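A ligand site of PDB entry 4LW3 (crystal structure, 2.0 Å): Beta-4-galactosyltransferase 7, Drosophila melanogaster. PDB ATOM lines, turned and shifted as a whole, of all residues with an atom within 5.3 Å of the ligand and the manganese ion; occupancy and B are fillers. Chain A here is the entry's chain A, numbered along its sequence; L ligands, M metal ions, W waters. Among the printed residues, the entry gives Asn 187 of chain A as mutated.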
ATOM      1  N   VAL A  57     -16.399   4.186 -22.933  1.00  0.00           N
ATOM      2  CA  VAL A  57     -16.861   3.857 -24.274  1.00  0.00           C
ATOM      3  C   VAL A  57     -15.984   2.768 -24.888  1.00  0.00           C
ATOM      4  O   VAL A  57     -14.941   3.078 -25.480  1.00  0.00           O
ATOM      5  CB  VAL A  57     -16.798   5.076 -25.212  1.00  0.00           C
ATOM      6  CG1 VAL A  57     -17.446   4.742 -26.562  1.00  0.00           C
ATOM      7  CG2 VAL A  57     -17.490   6.284 -24.581  1.00  0.00           C
ATOM      8  N   PRO A  58     -16.393   1.503 -24.720  1.00  0.00           N
ATOM      9  CA  PRO A  58     -15.707   0.391 -25.399  1.00  0.00           C
ATOM     10  C   PRO A  58     -15.710   0.663 -26.878  1.00  0.00           C
ATOM     11  O   PRO A  58     -16.713   1.141 -27.424  1.00  0.00           O
ATOM     12  CB  PRO A  58     -16.577  -0.835 -25.064  1.00  0.00           C
ATOM     13  CG  PRO A  58     -17.822  -0.305 -24.356  1.00  0.00           C
ATOM     14  CD  PRO A  58     -17.476   1.053 -23.825  1.00  0.00           C
ATOM     15  N   PHE A  59     -14.589   0.403 -27.540  1.00  0.00           N
ATOM     16  CA  PHE A  59     -14.402   0.956 -28.868  1.00  0.00           C
ATOM     17  C   PHE A  59     -13.445   0.129 -29.709  1.00  0.00           C
ATOM     18  O   PHE A  59     -12.405  -0.320 -29.227  1.00  0.00           O
ATOM     19  CB  PHE A  59     -13.839   2.366 -28.703  1.00  0.00           C
ATOM     20  CG  PHE A  59     -13.638   3.113 -29.994  1.00  0.00           C
ATOM     21  CD1 PHE A  59     -12.477   2.952 -30.740  1.00  0.00           C
ATOM     22  CD2 PHE A  59     -14.610   3.999 -30.445  1.00  0.00           C
ATOM     23  CE1 PHE A  59     -12.294   3.635 -31.933  1.00  0.00           C
ATOM     24  CE2 PHE A  59     -14.437   4.692 -31.633  1.00  0.00           C
ATOM     25  CZ  PHE A  59     -13.274   4.521 -32.378  1.00  0.00           C
ATOM     26  N   ARG A  60     -13.845  -0.084 -30.962  1.00  0.00           N
ATOM     27  CA  ARG A  60     -12.926  -0.546 -32.007  1.00  0.00           C
ATOM     28  C   ARG A  60     -13.536  -0.237 -33.359  1.00  0.00           C
ATOM     29  O   ARG A  60     -14.688  -0.603 -33.643  1.00  0.00           O
ATOM     30  CB  ARG A  60     -12.625  -2.034 -31.889  1.00  0.00           C
ATOM     31  CG  ARG A  60     -11.833  -2.580 -33.084  1.00  0.00           C
ATOM     32  CD  ARG A  60     -11.979  -4.079 -33.186  1.00  0.00           C
ATOM     33  NE  ARG A  60     -10.982  -4.744 -32.348  1.00  0.00           N
ATOM     34  CZ  ARG A  60     -11.011  -6.030 -32.029  1.00  0.00           C
ATOM     35  NH1 ARG A  60     -12.000  -6.814 -32.440  1.00  0.00           N
ATOM     36  NH2 ARG A  60     -10.041  -6.527 -31.271  1.00  0.00           N
ATOM     37  N   ASP A  61     -12.770   0.461 -34.193  1.00  0.00           N
ATOM     38  CA  ASP A  61     -13.181   0.763 -35.569  1.00  0.00           C
ATOM     39  C   ASP A  61     -14.513   1.528 -35.665  1.00  0.00           C
ATOM     40  O   ASP A  61     -15.347   1.199 -36.493  1.00  0.00           O
ATOM     41  CB  ASP A  61     -13.314  -0.540 -36.373  1.00  0.00           C
ATOM     42  CG  ASP A  61     -11.989  -1.296 -36.509  1.00  0.00           C
ATOM     43  OD1 ASP A  61     -10.914  -0.680 -36.391  1.00  0.00           O
ATOM     44  OD2 ASP A  61     -12.045  -2.527 -36.730  1.00  0.00           O
ATOM     45  N   ARG A  62     -14.698   2.551 -34.820  1.00  0.00           N
ATOM     46  CA  ARG A  62     -15.919   3.353 -34.869  1.00  0.00           C
ATOM     47  C   ARG A  62     -15.592   4.837 -34.814  1.00  0.00           C
ATOM     48  O   ARG A  62     -16.266   5.603 -34.138  1.00  0.00           O
ATOM     49  CB  ARG A  62     -16.866   2.993 -33.716  1.00  0.00           C
ATOM     50  CG  ARG A  62     -17.309   1.539 -33.689  1.00  0.00           C
ATOM     51  CD  ARG A  62     -18.195   1.200 -34.903  1.00  0.00           C
ATOM     52  NE  ARG A  62     -18.680  -0.175 -34.840  1.00  0.00           N
ATOM     53  CZ  ARG A  62     -18.104  -1.216 -35.440  1.00  0.00           C
ATOM     54  NH1 ARG A  62     -17.008  -1.028 -36.169  1.00  0.00           N
ATOM     55  NH2 ARG A  62     -18.613  -2.425 -35.327  1.00  0.00           N
ATOM     56  N   PHE A  97     -14.277  -8.633 -30.524  1.00  0.00           N
ATOM     57  CA  PHE A  97     -14.593  -7.500 -29.672  1.00  0.00           C
ATOM     58  C   PHE A  97     -15.164  -7.926 -28.313  1.00  0.00           C
ATOM     59  O   PHE A  97     -16.162  -8.649 -28.265  1.00  0.00           O
ATOM     60  CB  PHE A  97     -15.570  -6.566 -30.380  1.00  0.00           C
ATOM     61  CG  PHE A  97     -15.746  -5.254 -29.688  1.00  0.00           C
ATOM     62  CD1 PHE A  97     -14.702  -4.343 -29.629  1.00  0.00           C
ATOM     63  CD2 PHE A  97     -16.953  -4.936 -29.080  1.00  0.00           C
ATOM     64  CE1 PHE A  97     -14.855  -3.125 -28.980  1.00  0.00           C
ATOM     65  CE2 PHE A  97     -17.107  -3.715 -28.417  1.00  0.00           C
ATOM     66  CZ  PHE A  97     -16.054  -2.814 -28.363  1.00  0.00           C
ATOM     67  N   ARG A  99     -16.483  -6.061 -25.217  1.00  0.00           N
ATOM     68  CA  ARG A  99     -16.758  -4.757 -24.600  1.00  0.00           C
ATOM     69  C   ARG A  99     -16.709  -4.819 -23.074  1.00  0.00           C
ATOM     70  O   ARG A  99     -16.302  -3.855 -22.428  1.00  0.00           O
ATOM     71  CB  ARG A  99     -18.093  -4.170 -25.100  1.00  0.00           C
ATOM     72  CG  ARG A  99     -19.342  -4.810 -24.541  1.00  0.00           C
ATOM     73  CD  ARG A  99     -20.613  -4.140 -25.113  1.00  0.00           C
ATOM     74  NE  ARG A  99     -20.869  -2.813 -24.583  1.00  0.00           N
ATOM     75  CZ  ARG A  99     -21.479  -2.585 -23.416  1.00  0.00           C
ATOM     76  NH1 ARG A  99     -21.868  -3.601 -22.657  1.00  0.00           N
ATOM     77  NH2 ARG A  99     -21.690  -1.355 -22.985  1.00  0.00           N
ATOM     78  N   HIS A 120     -21.295   3.028 -22.003  1.00  0.00           N
ATOM     79  CA  HIS A 120     -22.038   3.733 -23.050  1.00  0.00           C
ATOM     80  C   HIS A 120     -21.653   3.266 -24.455  1.00  0.00           C
ATOM     81  O   HIS A 120     -20.482   3.324 -24.816  1.00  0.00           O
ATOM     82  CB  HIS A 120     -21.704   5.218 -22.922  1.00  0.00           C
ATOM     83  CG  HIS A 120     -22.829   6.139 -23.289  1.00  0.00           C
ATOM     84  ND1 HIS A 120     -23.384   6.194 -24.548  1.00  0.00           N
ATOM     85  CD2 HIS A 120     -23.479   7.082 -22.551  1.00  0.00           C
ATOM     86  CE1 HIS A 120     -24.334   7.112 -24.569  1.00  0.00           C
ATOM     87  NE2 HIS A 120     -24.416   7.658 -23.371  1.00  0.00           N
ATOM     88  N   ASP A 121     -22.630   2.802 -25.251  1.00  0.00           N
ATOM     89  CA  ASP A 121     -22.382   2.514 -26.665  1.00  0.00           C
ATOM     90  C   ASP A 121     -22.048   3.824 -27.385  1.00  0.00           C
ATOM     91  O   ASP A 121     -22.605   4.873 -27.049  1.00  0.00           O
ATOM     92  CB  ASP A 121     -23.601   1.889 -27.330  1.00  0.00           C
ATOM     93  CG  ASP A 121     -23.978   0.543 -26.747  1.00  0.00           C
ATOM     94  OD1 ASP A 121     -23.207   0.021 -25.904  1.00  0.00           O
ATOM     95  OD2 ASP A 121     -25.041   0.005 -27.130  1.00  0.00           O
ATOM     96  N   VAL A 122     -21.171   3.761 -28.379  1.00  0.00           N
ATOM     97  CA  VAL A 122     -20.722   4.976 -29.045  1.00  0.00           C
ATOM     98  C   VAL A 122     -21.748   5.489 -30.064  1.00  0.00           C
ATOM     99  O   VAL A 122     -21.680   6.642 -30.506  1.00  0.00           O
ATOM    100  CB  VAL A 122     -19.357   4.748 -29.737  1.00  0.00           C
ATOM    101  CG1 VAL A 122     -19.551   3.963 -31.029  1.00  0.00           C
ATOM    102  CG2 VAL A 122     -18.646   6.076 -30.003  1.00  0.00           C
ATOM    103  N   ASP A 123     -22.716   4.644 -30.422  1.00  0.00           N
ATOM    104  CA  ASP A 123     -23.652   4.959 -31.507  1.00  0.00           C
ATOM    105  C   ASP A 123     -25.054   5.321 -30.993  1.00  0.00           C
ATOM    106  O   ASP A 123     -26.015   5.425 -31.779  1.00  0.00           O
ATOM    107  CB  ASP A 123     -23.784   3.751 -32.444  1.00  0.00           C
ATOM    108  CG  ASP A 123     -24.301   2.521 -31.719  1.00  0.00           C
ATOM    109  OD1 ASP A 123     -24.623   2.634 -30.511  1.00  0.00           O
ATOM    110  OD2 ASP A 123     -24.395   1.434 -32.342  1.00  0.00           O
ATOM    111  N   LEU A 124     -25.174   5.495 -29.687  1.00  0.00           N
ATOM    112  CA  LEU A 124     -26.488   5.652 -29.067  1.00  0.00           C
ATOM    113  C   LEU A 124     -26.571   6.987 -28.337  1.00  0.00           C
ATOM    114  O   LEU A 124     -25.960   7.152 -27.274  1.00  0.00           O
ATOM    115  CB  LEU A 124     -26.752   4.481 -28.102  1.00  0.00           C
ATOM    116  CG  LEU A 124     -28.160   4.392 -27.496  1.00  0.00           C
ATOM    117  CD1 LEU A 124     -29.185   4.185 -28.599  1.00  0.00           C
ATOM    118  CD2 LEU A 124     -28.226   3.255 -26.474  1.00  0.00           C
ATOM    119  N   HIS A 150     -35.728   2.396 -25.734  1.00  0.00           N
ATOM    120  CA  HIS A 150     -34.735   1.998 -26.712  1.00  0.00           C
ATOM    121  C   HIS A 150     -35.399   1.663 -28.049  1.00  0.00           C
ATOM    122  O   HIS A 150     -36.470   1.058 -28.081  1.00  0.00           O
ATOM    123  CB  HIS A 150     -33.912   0.814 -26.204  1.00  0.00           C
ATOM    124  CG  HIS A 150     -32.651   0.574 -26.993  1.00  0.00           C
ATOM    125  ND1 HIS A 150     -32.638  -0.099 -28.193  1.00  0.00           N
ATOM    126  CD2 HIS A 150     -31.365   0.939 -26.749  1.00  0.00           C
ATOM    127  CE1 HIS A 150     -31.407  -0.138 -28.664  1.00  0.00           C
ATOM    128  NE2 HIS A 150     -30.613   0.485 -27.808  1.00  0.00           N
ATOM    129  N   TYR A 153     -34.264  -2.710 -28.566  1.00  0.00           N
ATOM    130  CA  TYR A 153     -34.319  -3.754 -27.554  1.00  0.00           C
ATOM    131  C   TYR A 153     -35.398  -3.427 -26.529  1.00  0.00           C
ATOM    132  O   TYR A 153     -35.357  -2.378 -25.880  1.00  0.00           O
ATOM    133  CB  TYR A 153     -32.947  -3.963 -26.891  1.00  0.00           C
ATOM    134  CG  TYR A 153     -31.894  -4.394 -27.893  1.00  0.00           C
ATOM    135  CD1 TYR A 153     -31.922  -5.656 -28.466  1.00  0.00           C
ATOM    136  CD2 TYR A 153     -30.875  -3.528 -28.284  1.00  0.00           C
ATOM    137  CE1 TYR A 153     -30.957  -6.051 -29.383  1.00  0.00           C
ATOM    138  CE2 TYR A 153     -29.921  -3.904 -29.197  1.00  0.00           C
ATOM    139  CZ  TYR A 153     -29.957  -5.175 -29.749  1.00  0.00           C
ATOM    140  OH  TYR A 153     -29.009  -5.553 -30.670  1.00  0.00           O
ATOM    141  N   PHE A 158     -33.520  -5.939 -20.283  1.00  0.00           N
ATOM    142  CA  PHE A 158     -32.482  -5.287 -21.070  1.00  0.00           C
ATOM    143  C   PHE A 158     -31.849  -4.166 -20.255  1.00  0.00           C
ATOM    144  O   PHE A 158     -32.543  -3.283 -19.752  1.00  0.00           O
ATOM    145  CB  PHE A 158     -33.100  -4.691 -22.340  1.00  0.00           C
ATOM    146  CG  PHE A 158     -32.136  -3.872 -23.156  1.00  0.00           C
ATOM    147  CD1 PHE A 158     -31.123  -4.490 -23.891  1.00  0.00           C
ATOM    148  CD2 PHE A 158     -32.247  -2.494 -23.209  1.00  0.00           C
ATOM    149  CE1 PHE A 158     -30.238  -3.732 -24.667  1.00  0.00           C
ATOM    150  CE2 PHE A 158     -31.368  -1.714 -23.973  1.00  0.00           C
ATOM    151  CZ  PHE A 158     -30.353  -2.342 -24.707  1.00  0.00           C
ATOM    152  N   GLY A 160     -28.743  -2.731 -21.528  1.00  0.00           N
ATOM    153  CA  GLY A 160     -27.635  -2.353 -22.384  1.00  0.00           C
ATOM    154  C   GLY A 160     -27.676  -0.918 -22.871  1.00  0.00           C
ATOM    155  O   GLY A 160     -28.501  -0.117 -22.412  1.00  0.00           O
ATOM    156  N   GLY A 161     -26.784  -0.580 -23.807  1.00  0.00           N
ATOM    157  CA  GLY A 161     -26.782   0.749 -24.378  1.00  0.00           C
ATOM    158  C   GLY A 161     -26.128   1.801 -23.495  1.00  0.00           C
ATOM    159  O   GLY A 161     -25.033   2.283 -23.797  1.00  0.00           O
ATOM    160  N   GLY A 182     -17.084 -11.205 -28.893  1.00  0.00           N
ATOM    161  CA  GLY A 182     -18.075 -11.102 -29.955  1.00  0.00           C
ATOM    162  C   GLY A 182     -19.383 -10.559 -29.370  1.00  0.00           C
ATOM    163  O   GLY A 182     -19.506 -10.389 -28.164  1.00  0.00           O
ATOM    164  N   TRP A 183     -20.351 -10.304 -30.245  1.00  0.00           N
ATOM    165  CA  TRP A 183     -21.608  -9.672 -29.829  1.00  0.00           C
ATOM    166  C   TRP A 183     -22.429 -10.502 -28.836  1.00  0.00           C
ATOM    167  O   TRP A 183     -22.470 -11.741 -28.911  1.00  0.00           O
ATOM    168  CB  TRP A 183     -22.474  -9.375 -31.068  1.00  0.00           C
ATOM    169  CG  TRP A 183     -23.788  -8.671 -30.732  1.00  0.00           C
ATOM    170  CD1 TRP A 183     -24.031  -7.320 -30.726  1.00  0.00           C
ATOM    171  CD2 TRP A 183     -25.028  -9.303 -30.352  1.00  0.00           C
ATOM    172  NE1 TRP A 183     -25.343  -7.076 -30.367  1.00  0.00           N
ATOM    173  CE2 TRP A 183     -25.973  -8.280 -30.133  1.00  0.00           C
ATOM    174  CE3 TRP A 183     -25.424 -10.628 -30.190  1.00  0.00           C
ATOM    175  CZ2 TRP A 183     -27.293  -8.547 -29.754  1.00  0.00           C
ATOM    176  CZ3 TRP A 183     -26.728 -10.902 -29.808  1.00  0.00           C
ATOM    177  CH2 TRP A 183     -27.648  -9.864 -29.588  1.00  0.00           C
ATOM    178  N   GLY A 184     -23.067  -9.796 -27.898  1.00  0.00           N
ATOM    179  CA  GLY A 184     -24.184 -10.333 -27.133  1.00  0.00           C
ATOM    180  C   GLY A 184     -23.941 -10.827 -25.728  1.00  0.00           C
ATOM    181  O   GLY A 184     -22.808 -11.140 -25.357  1.00  0.00           O
ATOM    182  N   LEU A 185     -25.021 -10.872 -24.949  1.00  0.00           N
ATOM    183  CA  LEU A 185     -25.120 -11.557 -23.652  1.00  0.00           C
ATOM    184  C   LEU A 185     -24.390 -10.940 -22.445  1.00  0.00           C
ATOM    185  O   LEU A 185     -24.768 -11.204 -21.295  1.00  0.00           O
ATOM    186  CB  LEU A 185     -24.747 -13.046 -23.798  1.00  0.00           C
ATOM    187  CG  LEU A 185     -25.713 -13.920 -24.604  1.00  0.00           C
ATOM    188  CD1 LEU A 185     -25.206 -15.356 -24.688  1.00  0.00           C
ATOM    189  CD2 LEU A 185     -27.112 -13.883 -23.989  1.00  0.00           C
ATOM    190  N   GLU A 186     -23.350 -10.142 -22.690  1.00  0.00           N
ATOM    191  CA  GLU A 186     -22.540  -9.666 -21.572  1.00  0.00           C
ATOM    192  C   GLU A 186     -23.325  -8.788 -20.593  1.00  0.00           C
ATOM    193  O   GLU A 186     -23.093  -8.838 -19.382  1.00  0.00           O
ATOM    194  CB  GLU A 186     -21.261  -8.959 -22.056  1.00  0.00           C
ATOM    195  CG  GLU A 186     -21.395  -7.470 -22.317  1.00  0.00           C
ATOM    196  CD  GLU A 186     -22.245  -7.156 -23.535  1.00  0.00           C
ATOM    197  OE1 GLU A 186     -22.327  -8.004 -24.455  1.00  0.00           O
ATOM    198  OE2 GLU A 186     -22.818  -6.048 -23.580  1.00  0.00           O
ATOM    199  N   ASN A 187     -24.264  -7.996 -21.108  1.00  0.00           N
ATOM    200  CA  ASN A 187     -25.073  -7.127 -20.238  1.00  0.00           C
ATOM    201  C   ASN A 187     -26.140  -7.926 -19.517  1.00  0.00           C
ATOM    202  O   ASN A 187     -26.566  -7.569 -18.413  1.00  0.00           O
ATOM    203  CB  ASN A 187     -25.704  -5.988 -21.040  1.00  0.00           C
ATOM    204  CG  ASN A 187     -24.869  -4.733 -21.031  1.00  0.00           C
ATOM    205  OD1 ASN A 187     -24.261  -4.390 -20.017  1.00  0.00           O
ATOM    206  ND2 ASN A 187     -24.831  -4.016 -22.160  1.00  0.00           N
ATOM    207  N   HIS A 217     -30.160   5.852 -32.622  1.00  0.00           N
ATOM    208  CA  HIS A 217     -29.292   4.686 -32.727  1.00  0.00           C
ATOM    209  C   HIS A 217     -28.877   4.558 -34.173  1.00  0.00           C
ATOM    210  O   HIS A 217     -29.554   3.904 -34.968  1.00  0.00           O
ATOM    211  CB  HIS A 217     -30.009   3.411 -32.288  1.00  0.00           C
ATOM    212  CG  HIS A 217     -29.121   2.193 -32.277  1.00  0.00           C
ATOM    213  ND1 HIS A 217     -29.608   0.919 -32.527  1.00  0.00           N
ATOM    214  CD2 HIS A 217     -27.798   2.051 -32.037  1.00  0.00           C
ATOM    215  CE1 HIS A 217     -28.616   0.049 -32.434  1.00  0.00           C
ATOM    216  NE2 HIS A 217     -27.503   0.707 -32.137  1.00  0.00           N
ATOM    217  N   HIS A 219     -26.886   2.883 -36.417  1.00  0.00           N
ATOM    218  CA  HIS A 219     -26.130   1.649 -36.493  1.00  0.00           C
ATOM    219  C   HIS A 219     -26.809   0.822 -37.576  1.00  0.00           C
ATOM    220  O   HIS A 219     -27.830   0.191 -37.341  1.00  0.00           O
ATOM    221  CB  HIS A 219     -26.186   0.906 -35.148  1.00  0.00           C
ATOM    222  CG  HIS A 219     -25.454  -0.402 -35.132  1.00  0.00           C
ATOM    223  ND1 HIS A 219     -25.230  -1.116 -33.963  1.00  0.00           N
ATOM    224  CD2 HIS A 219     -24.900  -1.131 -36.128  1.00  0.00           C
ATOM    225  CE1 HIS A 219     -24.571  -2.223 -34.259  1.00  0.00           C
ATOM    226  NE2 HIS A 219     -24.356  -2.256 -35.562  1.00  0.00           N
ATOM    227  N   LYS A 225     -21.242  -4.583 -38.710  1.00  0.00           N
ATOM    228  CA  LYS A 225     -21.828  -5.902 -38.479  1.00  0.00           C
ATOM    229  C   LYS A 225     -21.712  -6.330 -37.019  1.00  0.00           C
ATOM    230  O   LYS A 225     -20.741  -5.996 -36.338  1.00  0.00           O
ATOM    231  CB  LYS A 225     -21.188  -6.970 -39.369  1.00  0.00           C
ATOM    232  CG  LYS A 225     -21.679  -6.917 -40.807  1.00  0.00           C
ATOM    233  CD  LYS A 225     -21.053  -8.012 -41.653  1.00  0.00           C
ATOM    234  CE  LYS A 225     -21.545  -7.959 -43.090  1.00  0.00           C
ATOM    235  NZ  LYS A 225     -21.354  -6.610 -43.697  1.00  0.00           N
ATOM    236  N   ARG A 226     -22.728  -7.041 -36.544  1.00  0.00           N
ATOM    237  CA  ARG A 226     -22.667  -7.664 -35.234  1.00  0.00           C
ATOM    238  C   ARG A 226     -21.969  -9.010 -35.376  1.00  0.00           C
ATOM    239  O   ARG A 226     -22.348  -9.830 -36.215  1.00  0.00           O
ATOM    240  CB  ARG A 226     -24.073  -7.826 -34.648  1.00  0.00           C
ATOM    241  CG  ARG A 226     -24.757  -6.495 -34.330  1.00  0.00           C
ATOM    242  CD  ARG A 226     -26.191  -6.678 -33.781  1.00  0.00           C
ATOM    243  NE  ARG A 226     -26.706  -5.391 -33.337  1.00  0.00           N
ATOM    244  CZ  ARG A 226     -27.302  -4.501 -34.135  1.00  0.00           C
ATOM    245  NH1 ARG A 226     -27.474  -4.780 -35.430  1.00  0.00           N
ATOM    246  NH2 ARG A 226     -27.724  -3.335 -33.651  1.00  0.00           N
HETATM  247  N1  LIG L   1     -18.425  -1.587 -30.520  1.00  0.00           N
HETATM  248  C1  LIG L   1     -17.295  -1.216 -31.157  1.00  0.00           C
HETATM  249  N2  LIG L   1     -16.762  -1.981 -32.088  1.00  0.00           N
HETATM  250  C2  LIG L   1     -17.315  -3.166 -32.427  1.00  0.00           C
HETATM  251  C3  LIG L   1     -18.491  -3.606 -31.774  1.00  0.00           C
HETATM  252  C4  LIG L   1     -19.041  -2.745 -30.792  1.00  0.00           C
HETATM  253  O1  LIG L   1     -16.772  -0.168 -30.885  1.00  0.00           O
HETATM  254  O2  LIG L   1     -16.723  -3.979 -33.416  1.00  0.00           O
HETATM  255  C5  LIG L   1     -18.958  -0.783 -29.523  1.00  0.00           C
HETATM  256  C6  LIG L   1     -19.741   0.442 -30.009  1.00  0.00           C
HETATM  257  O3  LIG L   1     -19.594   1.460 -29.057  1.00  0.00           O
HETATM  258  C7  LIG L   1     -21.121  -0.075 -30.032  1.00  0.00           C
HETATM  259  C8  LIG L   1     -21.149  -0.875 -28.771  1.00  0.00           C
HETATM  260  O4  LIG L   1     -19.865  -1.561 -28.711  1.00  0.00           O
HETATM  261  O5  LIG L   1     -22.102   0.952 -30.034  1.00  0.00           O
HETATM  262  C9  LIG L   1     -22.283  -1.883 -28.744  1.00  0.00           C
HETATM  263  O6  LIG L   1     -22.102  -2.822 -29.793  1.00  0.00           O
HETATM  264  P1  LIG L   1     -23.171  -2.866 -30.999  1.00  0.00           P
HETATM  265  O7  LIG L   1     -23.621  -1.434 -31.322  1.00  0.00           O
HETATM  266  O8  LIG L   1     -22.524  -3.530 -32.177  1.00  0.00           O
HETATM  267  O9  LIG L   1     -24.415  -3.790 -30.572  1.00  0.00           O
HETATM  268  P2  LIG L   1     -25.919  -3.401 -30.246  1.00  0.00           P
HETATM  269  O10 LIG L   1     -26.343  -2.250 -31.174  1.00  0.00           O
HETATM  270  O11 LIG L   1     -26.746  -4.653 -30.470  1.00  0.00           O
HETATM  271  O12 LIG L   1     -25.974  -2.907 -28.716  1.00  0.00           O
HETATM  272  C10 LIG L   1     -26.525  -3.708 -27.657  1.00  0.00           C
HETATM  273  C11 LIG L   1     -26.271  -3.060 -26.399  1.00  0.00           C
HETATM  274  C12 LIG L   1     -24.864  -3.027 -26.118  1.00  0.00           C
HETATM  275  C13 LIG L   1     -24.296  -4.387 -25.959  1.00  0.00           C
HETATM  276  C14 LIG L   1     -24.512  -5.327 -27.230  1.00  0.00           C
HETATM  277  C15 LIG L   1     -24.313  -6.648 -26.871  1.00  0.00           C
HETATM  278  O13 LIG L   1     -26.802  -1.632 -26.489  1.00  0.00           O
HETATM  279  O14 LIG L   1     -24.653  -2.234 -24.867  1.00  0.00           O
HETATM  280  O15 LIG L   1     -24.908  -5.027 -24.832  1.00  0.00           O
HETATM  281  O16 LIG L   1     -25.969  -5.071 -27.722  1.00  0.00           O
HETATM  282  O17 LIG L   1     -23.060  -6.959 -26.958  1.00  0.00           O
HETATM  283 MN    MN M   1     -25.505  -0.400 -31.855  1.00  0.00          MN
HETATM  284  O   HOH W   1     -17.308  -6.615 -33.584  1.00  0.00           O
HETATM  285  O   HOH W   2     -27.499  -5.959 -24.052  1.00  0.00           O
HETATM  286  O   HOH W   3     -21.012  -5.684 -30.986  1.00  0.00           O
HETATM  287  O   HOH W   4     -20.941  -0.909 -33.423  1.00  0.00           O
HETATM  288  O   HOH W   5     -28.202  -0.408 -28.638  1.00  0.00           O
HETATM  289  O   HOH W   6     -25.634   0.437 -29.727  1.00  0.00           O
HETATM  290  O   HOH W   7     -19.161   1.430 -26.682  1.00  0.00           O
HETATM  291  O   HOH W   8     -28.362  -6.189 -26.537  1.00  0.00           O
HETATM  292  O   HOH W   9     -20.520  -5.861 -28.265  1.00  0.00           O
HETATM  293  O   HOH W  10     -21.176  -3.703 -34.561  1.00  0.00           O
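NE1 of Trp 183 is in hydrogen-bond range of O11 of the ligand (2.8 Å). The backbone NH (N) of Arg 60 sits at hydrogen-bond distance from an oxygen (O1) of the ligand. NH2 of Arg 62 sits at hydrogen-bond distance from O2 of the ligand (3.1 Å). The backbone NH (N) of Val 122 lies within hydrogen-bond range of an oxygen (O3) of the ligand. N of Gly 161 is in hydrogen-bond range of O13 of the ligand (2.9 Å). O15 of the ligand lies within hydrogen-bond range of OE2 of Glu 186 (2.6 Å). The backbone carbonyl oxygen (O) of Pro 58 is in hydrogen-bond range of an oxygen (O3) of the ligand (3.3 Å). N of Gly 184 is in hydrogen-bond range of O17 of the ligand (3.0 Å). OD2 of Asp 121 is in hydrogen-bond range of O13 of the ligand. The guanidinium group (NE) of Arg 226 is in salt-bridge range of an oxygen (O11) of the ligand (3.0 Å). The backbone carbonyl oxygen of Arg 60 sits at hydrogen-bond distance from a nitrogen (N2) of the ligand, at 2.9 Å. The side-chain hydroxyl (OH) of Tyr 153 sits at hydrogen-bond distance from an oxygen (O11) of the ligand (2.4 Å). An oxygen (O15) of the ligand sits at hydrogen-bond distance from the side-chain amide nitrogen (ND2) of Asn 187 (2.9 Å).
OD1 of Asp 121 is in salt-bridge range of NH2 of Arg 99, at 3.6 Å. The guanidinium group of Arg 99 sits close to the side-chain amide nitrogen of Asn 187 (3.0 Å). ND2 of Asn 187 lies within hydrogen-bond range of OE2 of Glu 186, 3.2 Å away. The backbone carbonyl oxygen of Phe 97 is in hydrogen-bond range of the backbone NH of Gly 182 (2.8 Å). The backbone NH (N) of Asp 121 lies within hydrogen-bond range of the backbone carbonyl oxygen (O) of Gly 161, at 2.9 Å. The backbone carbonyl oxygen of Arg 60 sits close to the guanidinium group of Arg 62. The side-chain carboxylate of Glu 186 lies within salt-bridge range of the guanidinium group of Arg 99 (2.8 Å). A ring nitrogen (ND1) of His 219 sits close to the guanidinium group of Arg 226, 3.4 Å away.
Merely in contact with the ligand: Phe 97 (3.2 Å), Phe 59 (3.3 Å), Arg 99 (3.5 Å) and Gly 160 (3.8 Å). Hydrophobic or aromatic side chains within 4 Å of the ligand: Phe 97, Val 122, Tyr 153, Trp 183, His 217 and His 219. Within 4 Å of the ligand: Pro 58, Phe 59, Arg 60, Arg 62, Phe 97, Arg 99, Asp 121, Val 122, Asp 123, Tyr 153, Gly 160, Gly 161, Trp 183, Gly 184, Glu 186, Asn 187, His 217, His 219 and Arg 226. The nearest printed residue that does not touch the ligand is Phe 158 (4.04 Å).
The manganese ion is bound by an oxygen (O10) of the ligand (2.1 Å), the side-chain carboxylate (OD2) of Asp 123 (2.2 Å), an oxygen (O7) of the ligand (2.2 Å), a ring nitrogen (ND1) of His 219 (2.2 Å), water W6 (2.3 Å) and a ring nitrogen (NE2) of His 217 (2.3 Å).
Water W6 lies within hydrogen-bond range of the side-chain carboxylate of Asp 123 (2.5 Å) and the side-chain carboxylate of Asp 121 (2.7 Å). Water W7 lies within hydrogen-bond range of an oxygen (O3) of the ligand, the backbone carbonyl oxygen of Pro 58 and the backbone carbonyl oxygen of His 120. Water W10 lies within hydrogen-bond range of an oxygen (O8) of the ligand, the backbone carbonyl oxygen of Lys 225 and the guanidinium group of Arg 62. Water W5 lies within hydrogen-bond range of NE2 of His 150 and O13 of the ligand. Water W4 lies within hydrogen-bond range of NE of Arg 62 (2.8 Å) and O8 of the ligand (3.3 Å).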
